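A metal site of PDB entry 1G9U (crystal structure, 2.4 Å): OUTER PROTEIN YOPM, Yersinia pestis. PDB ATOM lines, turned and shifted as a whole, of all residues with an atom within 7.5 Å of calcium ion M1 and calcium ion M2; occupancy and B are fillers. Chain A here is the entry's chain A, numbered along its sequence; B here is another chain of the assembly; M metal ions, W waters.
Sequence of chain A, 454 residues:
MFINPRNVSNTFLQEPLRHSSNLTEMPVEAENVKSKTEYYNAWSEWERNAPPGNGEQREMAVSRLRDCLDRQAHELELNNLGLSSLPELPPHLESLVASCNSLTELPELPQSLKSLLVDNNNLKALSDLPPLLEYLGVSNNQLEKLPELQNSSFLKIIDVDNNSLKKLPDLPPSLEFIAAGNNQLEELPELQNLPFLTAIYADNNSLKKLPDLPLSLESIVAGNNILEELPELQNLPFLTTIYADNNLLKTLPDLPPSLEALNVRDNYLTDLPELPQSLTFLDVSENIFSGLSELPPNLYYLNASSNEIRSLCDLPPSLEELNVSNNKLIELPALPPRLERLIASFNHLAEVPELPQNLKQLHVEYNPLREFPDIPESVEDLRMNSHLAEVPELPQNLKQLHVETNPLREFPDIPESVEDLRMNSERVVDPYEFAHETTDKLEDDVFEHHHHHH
Of the 25 residues printed, 3 come within 4 Å of calcium ion M2.
Calcium ion M2 is bound by water W4 (2.2 Å), the side-chain carboxylate of Asp 266 (2.3 Å), the side-chain amide oxygen of Asn 246 (2.4 Å), the side-chain amide oxygen of Asn 326 of chain B (2.4 Å), water W7 (2.5 Å) and water W5 (2.5 Å). Calcium ion M2 has six donor atoms within binding distance.
Of the 25 residues printed, 3 come within 4 Å of calcium ion M1. The nearest printed residue that does not touch calcium ion M1 is Lys 328 of chain B (4.1 Å).
NZ of Lys 328 of chain B sits at hydrogen-bond distance from O of Asp 266 (2.7 Å). OE2 of Glu 308 of chain B lies within salt-bridge range of NZ of Lys 328 of chain B, at 2.8 Å. The backbone NH (N) of Asp 266 lies close to the side-chain amide nitrogen (ND2) of Asn 287 of chain A, at 3.5 Å. The backbone carbonyl oxygen of Glu 286 sits close to the backbone NH of Asp 266 (3.1 Å). The side-chain amide nitrogen (ND2) of Asn 246 lies within hydrogen-bond range of the side-chain carboxylate (OD2) of Asp 245, 3.2 Å away. OD1 of Asn 307 of chain B lies close to O of Asn 287 of chain B. The backbone NH of Asn 326 of chain B lies close to the backbone carbonyl oxygen of Phe 346 of chain B (3.3 Å). The backbone NH (N) of Phe 289 of chain B sits at hydrogen-bond distance from the side-chain amide oxygen (OD1) of Asn 307 of chain B.
Water W2 lies within hydrogen-bond range of O of Asn 267 (2.5 Å) and O of Glu 286 (2.8 Å). Water W5 lies within hydrogen-bond range of O of Asn 327 of chain B and O of Phe 346 of chain B.
Calcium ion M1 is bound by the side-chain carboxylate of Glu 308 of chain B (2.4 Å), water W6 (2.4 Å), water W1 (2.4 Å), the backbone carbonyl oxygen of Asn 307 of chain B (2.5 Å), the side-chain carboxylate of Asp 266 (2.5 Å), water W2 (2.7 Å) and water W3 (2.8 Å).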
ATOM      1  N   ASN A 224      13.017   4.695  13.937  1.00  0.00           N
ATOM      2  CA  ASN A 224      13.697   5.722  14.724  1.00  0.00           C
ATOM      3  C   ASN A 224      15.102   6.042  14.233  1.00  0.00           C
ATOM      4  O   ASN A 224      16.062   6.018  15.018  1.00  0.00           O
ATOM      5  CB  ASN A 224      13.786   5.193  16.166  1.00  0.00           C
ATOM      6  CG  ASN A 224      13.463   6.284  17.184  1.00  0.00           C
ATOM      7  OD1 ASN A 224      13.913   6.227  18.341  1.00  0.00           O
ATOM      8  ND2 ASN A 224      12.743   7.328  16.768  1.00  0.00           N
ATOM      9  N   ASP A 245       8.979   2.949  11.263  1.00  0.00           N
ATOM     10  CA  ASP A 245       8.291   3.890  12.108  1.00  0.00           C
ATOM     11  C   ASP A 245       9.255   4.984  12.600  1.00  0.00           C
ATOM     12  O   ASP A 245      10.472   4.765  12.707  1.00  0.00           O
ATOM     13  CB  ASP A 245       7.824   3.163  13.385  1.00  0.00           C
ATOM     14  CG  ASP A 245       8.956   2.380  14.014  1.00  0.00           C
ATOM     15  OD1 ASP A 245       9.379   1.384  13.404  1.00  0.00           O
ATOM     16  OD2 ASP A 245       9.414   2.732  15.127  1.00  0.00           O
ATOM     17  N   ASN A 246       8.727   6.157  12.938  1.00  0.00           N
ATOM     18  CA  ASN A 246       9.542   7.196  13.523  1.00  0.00           C
ATOM     19  C   ASN A 246      10.743   7.597  12.682  1.00  0.00           C
ATOM     20  O   ASN A 246      11.896   7.612  13.136  1.00  0.00           O
ATOM     21  CB  ASN A 246      10.060   6.767  14.919  1.00  0.00           C
ATOM     22  CG  ASN A 246       8.938   6.708  15.939  1.00  0.00           C
ATOM     23  OD1 ASN A 246       8.244   7.673  16.268  1.00  0.00           O
ATOM     24  ND2 ASN A 246       8.663   5.532  16.498  1.00  0.00           N
ATOM     25  N   ASN A 247      10.510   8.000  11.444  1.00  0.00           N
ATOM     26  CA  ASN A 247      11.569   8.534  10.606  1.00  0.00           C
ATOM     27  C   ASN A 247      11.082   9.807   9.935  1.00  0.00           C
ATOM     28  O   ASN A 247      10.305  10.598  10.480  1.00  0.00           O
ATOM     29  CB  ASN A 247      11.993   7.500   9.571  1.00  0.00           C
ATOM     30  CG  ASN A 247      12.941   6.437  10.092  1.00  0.00           C
ATOM     31  OD1 ASN A 247      14.128   6.721  10.329  1.00  0.00           O
ATOM     32  ND2 ASN A 247      12.399   5.222  10.255  1.00  0.00           N
ATOM     33  N   ARG A 265       4.621   3.773  11.511  1.00  0.00           N
ATOM     34  CA  ARG A 265       4.012   4.668  12.490  1.00  0.00           C
ATOM     35  C   ARG A 265       4.782   5.952  12.746  1.00  0.00           C
ATOM     36  O   ARG A 265       5.998   5.892  12.981  1.00  0.00           O
ATOM     37  CB  ARG A 265       3.945   3.866  13.783  1.00  0.00           C
ATOM     38  CG  ARG A 265       3.975   4.722  15.041  1.00  0.00           C
ATOM     39  CD  ARG A 265       3.473   3.830  16.165  1.00  0.00           C
ATOM     40  NE  ARG A 265       3.641   4.361  17.498  1.00  0.00           N
ATOM     41  CZ  ARG A 265       2.554   4.622  18.246  1.00  0.00           C
ATOM     42  NH1 ARG A 265       1.333   4.381  17.765  1.00  0.00           N
ATOM     43  NH2 ARG A 265       2.742   5.104  19.469  1.00  0.00           N
ATOM     44  N   ASP A 266       4.113   7.106  12.733  1.00  0.00           N
ATOM     45  CA  ASP A 266       4.797   8.344  13.077  1.00  0.00           C
ATOM     46  C   ASP A 266       5.740   8.705  11.960  1.00  0.00           C
ATOM     47  O   ASP A 266       6.942   8.830  12.169  1.00  0.00           O
ATOM     48  CB  ASP A 266       5.539   8.301  14.443  1.00  0.00           C
ATOM     49  CG  ASP A 266       5.905   9.729  14.846  1.00  0.00           C
ATOM     50  OD1 ASP A 266       5.781  10.631  13.980  1.00  0.00           O
ATOM     51  OD2 ASP A 266       6.392  10.030  15.969  1.00  0.00           O
ATOM     52  N   ASN A 267       5.105   8.909  10.834  1.00  0.00           N
ATOM     53  CA  ASN A 267       5.849   9.537   9.736  1.00  0.00           C
ATOM     54  C   ASN A 267       4.926  10.653   9.207  1.00  0.00           C
ATOM     55  O   ASN A 267       4.049  11.091   9.974  1.00  0.00           O
ATOM     56  CB  ASN A 267       6.257   8.524   8.689  1.00  0.00           C
ATOM     57  CG  ASN A 267       7.546   7.802   9.008  1.00  0.00           C
ATOM     58  OD1 ASN A 267       8.674   8.304   8.882  1.00  0.00           O
ATOM     59  ND2 ASN A 267       7.425   6.570   9.457  1.00  0.00           N
ATOM     60  N   TYR A 268       5.093  11.079   7.953  1.00  0.00           N
ATOM     61  CA  TYR A 268       4.371  12.206   7.377  1.00  0.00           C
ATOM     62  C   TYR A 268       3.640  11.794   6.101  1.00  0.00           C
ATOM     63  O   TYR A 268       3.636  12.475   5.081  1.00  0.00           O
ATOM     64  CB  TYR A 268       5.286  13.377   7.024  1.00  0.00           C
ATOM     65  CG  TYR A 268       4.705  14.780   7.115  1.00  0.00           C
ATOM     66  CD1 TYR A 268       4.387  15.370   8.345  1.00  0.00           C
ATOM     67  CD2 TYR A 268       4.480  15.549   5.978  1.00  0.00           C
ATOM     68  CE1 TYR A 268       3.868  16.656   8.416  1.00  0.00           C
ATOM     69  CE2 TYR A 268       3.965  16.839   6.018  1.00  0.00           C
ATOM     70  CZ  TYR A 268       3.667  17.375   7.257  1.00  0.00           C
ATOM     71  OH  TYR A 268       3.152  18.649   7.333  1.00  0.00           O
ATOM     72  N   GLU A 286      -0.152   7.655  13.615  1.00  0.00           N
ATOM     73  CA  GLU A 286       0.663   8.844  13.730  1.00  0.00           C
ATOM     74  C   GLU A 286       1.328   9.305  12.435  1.00  0.00           C
ATOM     75  O   GLU A 286       2.499   9.675  12.249  1.00  0.00           O
ATOM     76  CB  GLU A 286       1.698   8.570  14.809  1.00  0.00           C
ATOM     77  CG  GLU A 286       1.229   8.667  16.252  1.00  0.00           C
ATOM     78  CD  GLU A 286       2.448   8.724  17.167  1.00  0.00           C
ATOM     79  OE1 GLU A 286       3.226   9.691  17.147  1.00  0.00           O
ATOM     80  OE2 GLU A 286       2.705   7.800  17.959  1.00  0.00           O
ATOM     81  N   ASN A 287       0.475   9.342  11.416  1.00  0.00           N
ATOM     82  CA  ASN A 287       0.811   9.851  10.081  1.00  0.00           C
ATOM     83  C   ASN A 287      -0.161  10.967   9.793  1.00  0.00           C
ATOM     84  O   ASN A 287      -0.709  11.648  10.676  1.00  0.00           O
ATOM     85  CB  ASN A 287       0.707   8.718   9.037  1.00  0.00           C
ATOM     86  CG  ASN A 287       2.082   8.048   9.040  1.00  0.00           C
ATOM     87  OD1 ASN A 287       2.981   8.588   8.389  1.00  0.00           O
ATOM     88  ND2 ASN A 287       2.243   6.985   9.823  1.00  0.00           N
ATOM     89  N   ILE A 288      -0.449  11.246   8.531  1.00  0.00           N
ATOM     90  CA  ILE A 288      -1.402  12.360   8.429  1.00  0.00           C
ATOM     91  C   ILE A 288      -2.528  11.992   7.451  1.00  0.00           C
ATOM     92  O   ILE A 288      -2.893  12.812   6.587  1.00  0.00           O
ATOM     93  CB  ILE A 288      -0.660  13.654   8.040  1.00  0.00           C
ATOM     94  CG1 ILE A 288       0.109  13.546   6.708  1.00  0.00           C
ATOM     95  CG2 ILE A 288       0.319  14.130   9.097  1.00  0.00           C
ATOM     96  CD1 ILE A 288       0.792  14.842   6.331  1.00  0.00           C
ATOM     97  N   ASN B 287      -0.820  18.437  15.532  1.00  0.00           N
ATOM     98  CA  ASN B 287      -1.112  19.112  14.264  1.00  0.00           C
ATOM     99  C   ASN B 287      -0.119  18.584  13.260  1.00  0.00           C
ATOM    100  O   ASN B 287       0.413  17.464  13.341  1.00  0.00           O
ATOM    101  CB  ASN B 287      -0.993  20.643  14.434  1.00  0.00           C
ATOM    102  CG  ASN B 287      -2.377  21.098  14.904  1.00  0.00           C
ATOM    103  OD1 ASN B 287      -3.242  21.249  14.047  1.00  0.00           O
ATOM    104  ND2 ASN B 287      -2.573  21.208  16.215  1.00  0.00           N
ATOM    105  N   ILE B 288       0.207  19.349  12.228  1.00  0.00           N
ATOM    106  CA  ILE B 288       1.176  18.682  11.348  1.00  0.00           C
ATOM    107  C   ILE B 288       2.324  19.646  11.014  1.00  0.00           C
ATOM    108  O   ILE B 288       2.723  19.754   9.840  1.00  0.00           O
ATOM    109  CB  ILE B 288       0.471  18.138  10.099  1.00  0.00           C
ATOM    110  CG1 ILE B 288      -0.262  19.222   9.284  1.00  0.00           C
ATOM    111  CG2 ILE B 288      -0.530  17.040  10.408  1.00  0.00           C
ATOM    112  CD1 ILE B 288      -0.928  18.660   8.039  1.00  0.00           C
ATOM    113  N   PHE B 289       2.866  20.371  12.001  1.00  0.00           N
ATOM    114  CA  PHE B 289       3.951  21.317  11.801  1.00  0.00           C
ATOM    115  C   PHE B 289       5.298  20.624  11.608  1.00  0.00           C
ATOM    116  O   PHE B 289       5.537  19.693  12.396  1.00  0.00           O
ATOM    117  CB  PHE B 289       4.190  22.246  13.019  1.00  0.00           C
ATOM    118  CG  PHE B 289       3.020  23.192  13.189  1.00  0.00           C
ATOM    119  CD1 PHE B 289       1.925  22.771  13.924  1.00  0.00           C
ATOM    120  CD2 PHE B 289       3.048  24.450  12.608  1.00  0.00           C
ATOM    121  CE1 PHE B 289       0.821  23.579  14.098  1.00  0.00           C
ATOM    122  CE2 PHE B 289       1.924  25.239  12.750  1.00  0.00           C
ATOM    123  CZ  PHE B 289       0.824  24.814  13.461  1.00  0.00           C
ATOM    124  N   SER B 306       3.947  16.053  19.735  1.00  0.00           N
ATOM    125  CA  SER B 306       3.347  15.245  18.709  1.00  0.00           C
ATOM    126  C   SER B 306       2.994  15.972  17.419  1.00  0.00           C
ATOM    127  O   SER B 306       1.865  15.785  16.974  1.00  0.00           O
ATOM    128  CB  SER B 306       2.039  14.585  19.233  1.00  0.00           C
ATOM    129  OG  SER B 306       2.515  13.825  20.356  1.00  0.00           O
ATOM    130  N   ASN B 307       3.947  16.706  16.878  1.00  0.00           N
ATOM    131  CA  ASN B 307       3.923  17.288  15.550  1.00  0.00           C
ATOM    132  C   ASN B 307       4.970  16.539  14.721  1.00  0.00           C
ATOM    133  O   ASN B 307       5.286  15.371  14.997  1.00  0.00           O
ATOM    134  CB  ASN B 307       4.134  18.790  15.534  1.00  0.00           C
ATOM    135  CG  ASN B 307       2.772  19.447  15.766  1.00  0.00           C
ATOM    136  OD1 ASN B 307       1.933  19.580  14.868  1.00  0.00           O
ATOM    137  ND2 ASN B 307       2.572  19.872  17.011  1.00  0.00           N
ATOM    138  N   GLU B 308       5.523  17.171  13.699  1.00  0.00           N
ATOM    139  CA  GLU B 308       6.567  16.471  12.947  1.00  0.00           C
ATOM    140  C   GLU B 308       7.752  17.435  12.977  1.00  0.00           C
ATOM    141  O   GLU B 308       8.364  17.680  11.945  1.00  0.00           O
ATOM    142  CB  GLU B 308       6.143  16.226  11.499  1.00  0.00           C
ATOM    143  CG  GLU B 308       6.973  15.226  10.728  1.00  0.00           C
ATOM    144  CD  GLU B 308       7.047  13.841  11.330  1.00  0.00           C
ATOM    145  OE1 GLU B 308       6.553  13.517  12.427  1.00  0.00           O
ATOM    146  OE2 GLU B 308       7.638  12.994  10.625  1.00  0.00           O
ATOM    147  N   ILE B 309       7.978  18.088  14.102  1.00  0.00           N
ATOM    148  CA  ILE B 309       8.988  19.142  14.060  1.00  0.00           C
ATOM    149  C   ILE B 309      10.424  18.624  14.002  1.00  0.00           C
ATOM    150  O   ILE B 309      10.801  17.687  14.714  1.00  0.00           O
ATOM    151  CB  ILE B 309       8.746  20.036  15.287  1.00  0.00           C
ATOM    152  CG1 ILE B 309       7.351  20.675  15.170  1.00  0.00           C
ATOM    153  CG2 ILE B 309       9.861  21.018  15.521  1.00  0.00           C
ATOM    154  CD1 ILE B 309       7.078  21.566  16.395  1.00  0.00           C
ATOM    155  N   SER B 325       7.551  17.253  23.209  1.00  0.00           N
ATOM    156  CA  SER B 325       7.695  15.783  23.245  1.00  0.00           C
ATOM    157  C   SER B 325       7.280  15.120  21.937  1.00  0.00           C
ATOM    158  O   SER B 325       6.372  15.591  21.257  1.00  0.00           O
ATOM    159  CB  SER B 325       6.763  15.258  24.364  1.00  0.00           C
ATOM    160  OG  SER B 325       7.058  13.938  24.769  1.00  0.00           O
ATOM    161  N   ASN B 326       7.905  14.011  21.586  1.00  0.00           N
ATOM    162  CA  ASN B 326       7.392  13.253  20.463  1.00  0.00           C
ATOM    163  C   ASN B 326       7.373  14.052  19.167  1.00  0.00           C
ATOM    164  O   ASN B 326       6.308  14.120  18.543  1.00  0.00           O
ATOM    165  CB  ASN B 326       5.990  12.726  20.804  1.00  0.00           C
ATOM    166  CG  ASN B 326       5.600  11.696  19.725  1.00  0.00           C
ATOM    167  OD1 ASN B 326       6.437  11.050  19.082  1.00  0.00           O
ATOM    168  ND2 ASN B 326       4.323  11.502  19.428  1.00  0.00           N
ATOM    169  N   ASN B 327       8.538  14.606  18.801  1.00  0.00           N
ATOM    170  CA  ASN B 327       8.722  15.318  17.546  1.00  0.00           C
ATOM    171  C   ASN B 327       9.886  14.678  16.790  1.00  0.00           C
ATOM    172  O   ASN B 327      10.175  13.531  17.043  1.00  0.00           O
ATOM    173  CB  ASN B 327       8.948  16.835  17.701  1.00  0.00           C
ATOM    174  CG  ASN B 327       7.609  17.528  17.797  1.00  0.00           C
ATOM    175  OD1 ASN B 327       6.982  17.706  16.736  1.00  0.00           O
ATOM    176  ND2 ASN B 327       7.199  17.853  19.036  1.00  0.00           N
ATOM    177  N   LYS B 328      10.546  15.394  15.886  1.00  0.00           N
ATOM    178  CA  LYS B 328      11.623  14.733  15.163  1.00  0.00           C
ATOM    179  C   LYS B 328      12.891  15.533  15.384  1.00  0.00           C
ATOM    180  O   LYS B 328      13.649  15.730  14.431  1.00  0.00           O
ATOM    181  CB  LYS B 328      11.293  14.685  13.674  1.00  0.00           C
ATOM    182  CG  LYS B 328      10.041  13.831  13.430  1.00  0.00           C
ATOM    183  CD  LYS B 328      10.317  12.378  13.708  1.00  0.00           C
ATOM    184  CE  LYS B 328       9.172  11.404  13.773  1.00  0.00           C
ATOM    185  NZ  LYS B 328       8.315  11.160  12.571  1.00  0.00           N
ATOM    186  N   SER B 345      10.974  14.618  25.802  1.00  0.00           N
ATOM    187  CA  SER B 345      10.842  13.182  25.674  1.00  0.00           C
ATOM    188  C   SER B 345      10.518  12.765  24.237  1.00  0.00           C
ATOM    189  O   SER B 345       9.843  13.458  23.476  1.00  0.00           O
ATOM    190  CB  SER B 345       9.711  12.740  26.630  1.00  0.00           C
ATOM    191  OG  SER B 345      10.305  12.394  27.867  1.00  0.00           O
ATOM    192  N   PHE B 346      10.955  11.566  23.853  1.00  0.00           N
ATOM    193  CA  PHE B 346      10.749  10.988  22.532  1.00  0.00           C
ATOM    194  C   PHE B 346      11.178  11.863  21.366  1.00  0.00           C
ATOM    195  O   PHE B 346      10.406  12.194  20.449  1.00  0.00           O
ATOM    196  CB  PHE B 346       9.284  10.569  22.262  1.00  0.00           C
ATOM    197  CG  PHE B 346       8.797   9.607  23.343  1.00  0.00           C
ATOM    198  CD1 PHE B 346       9.013   8.254  23.226  1.00  0.00           C
ATOM    199  CD2 PHE B 346       8.180  10.122  24.468  1.00  0.00           C
ATOM    200  CE1 PHE B 346       8.566   7.388  24.242  1.00  0.00           C
ATOM    201  CE2 PHE B 346       7.761   9.280  25.463  1.00  0.00           C
ATOM    202  CZ  PHE B 346       7.977   7.918  25.363  1.00  0.00           C
ATOM    203  N   ASN B 347      12.460  12.190  21.371  1.00  0.00           N
ATOM    204  CA  ASN B 347      12.961  12.878  20.165  1.00  0.00           C
ATOM    205  C   ASN B 347      14.261  12.156  19.770  1.00  0.00           C
ATOM    206  O   ASN B 347      14.554  11.065  20.278  1.00  0.00           O
ATOM    207  CB  ASN B 347      13.194  14.358  20.414  1.00  0.00           C
ATOM    208  CG  ASN B 347      11.936  15.180  20.174  1.00  0.00           C
ATOM    209  OD1 ASN B 347      11.537  15.373  19.035  1.00  0.00           O
ATOM    210  ND2 ASN B 347      11.368  15.594  21.309  1.00  0.00           N
HETATM  211 CA    CA M   1       4.940  13.035  14.071  1.00  0.00          CA
HETATM  212 CA    CA M   2       7.462   9.259  17.823  1.00  0.00          CA
HETATM  213  O   HOH W   1       6.409  13.082  16.007  1.00  0.00           O
HETATM  214  O   HOH W   2       3.306  12.325  12.040  1.00  0.00           O
HETATM  215  O   HOH W   3       2.782  14.431  12.846  1.00  0.00           O
HETATM  216  O   HOH W   4       8.476   8.376  19.515  1.00  0.00           O
HETATM  217  O   HOH W   5       9.356  10.896  17.610  1.00  0.00           O
HETATM  218  O   HOH W   6       3.290  12.252  15.621  1.00  0.00           O
HETATM  219  O   HOH W   7       5.426   7.865  18.143  1.00  0.00           O
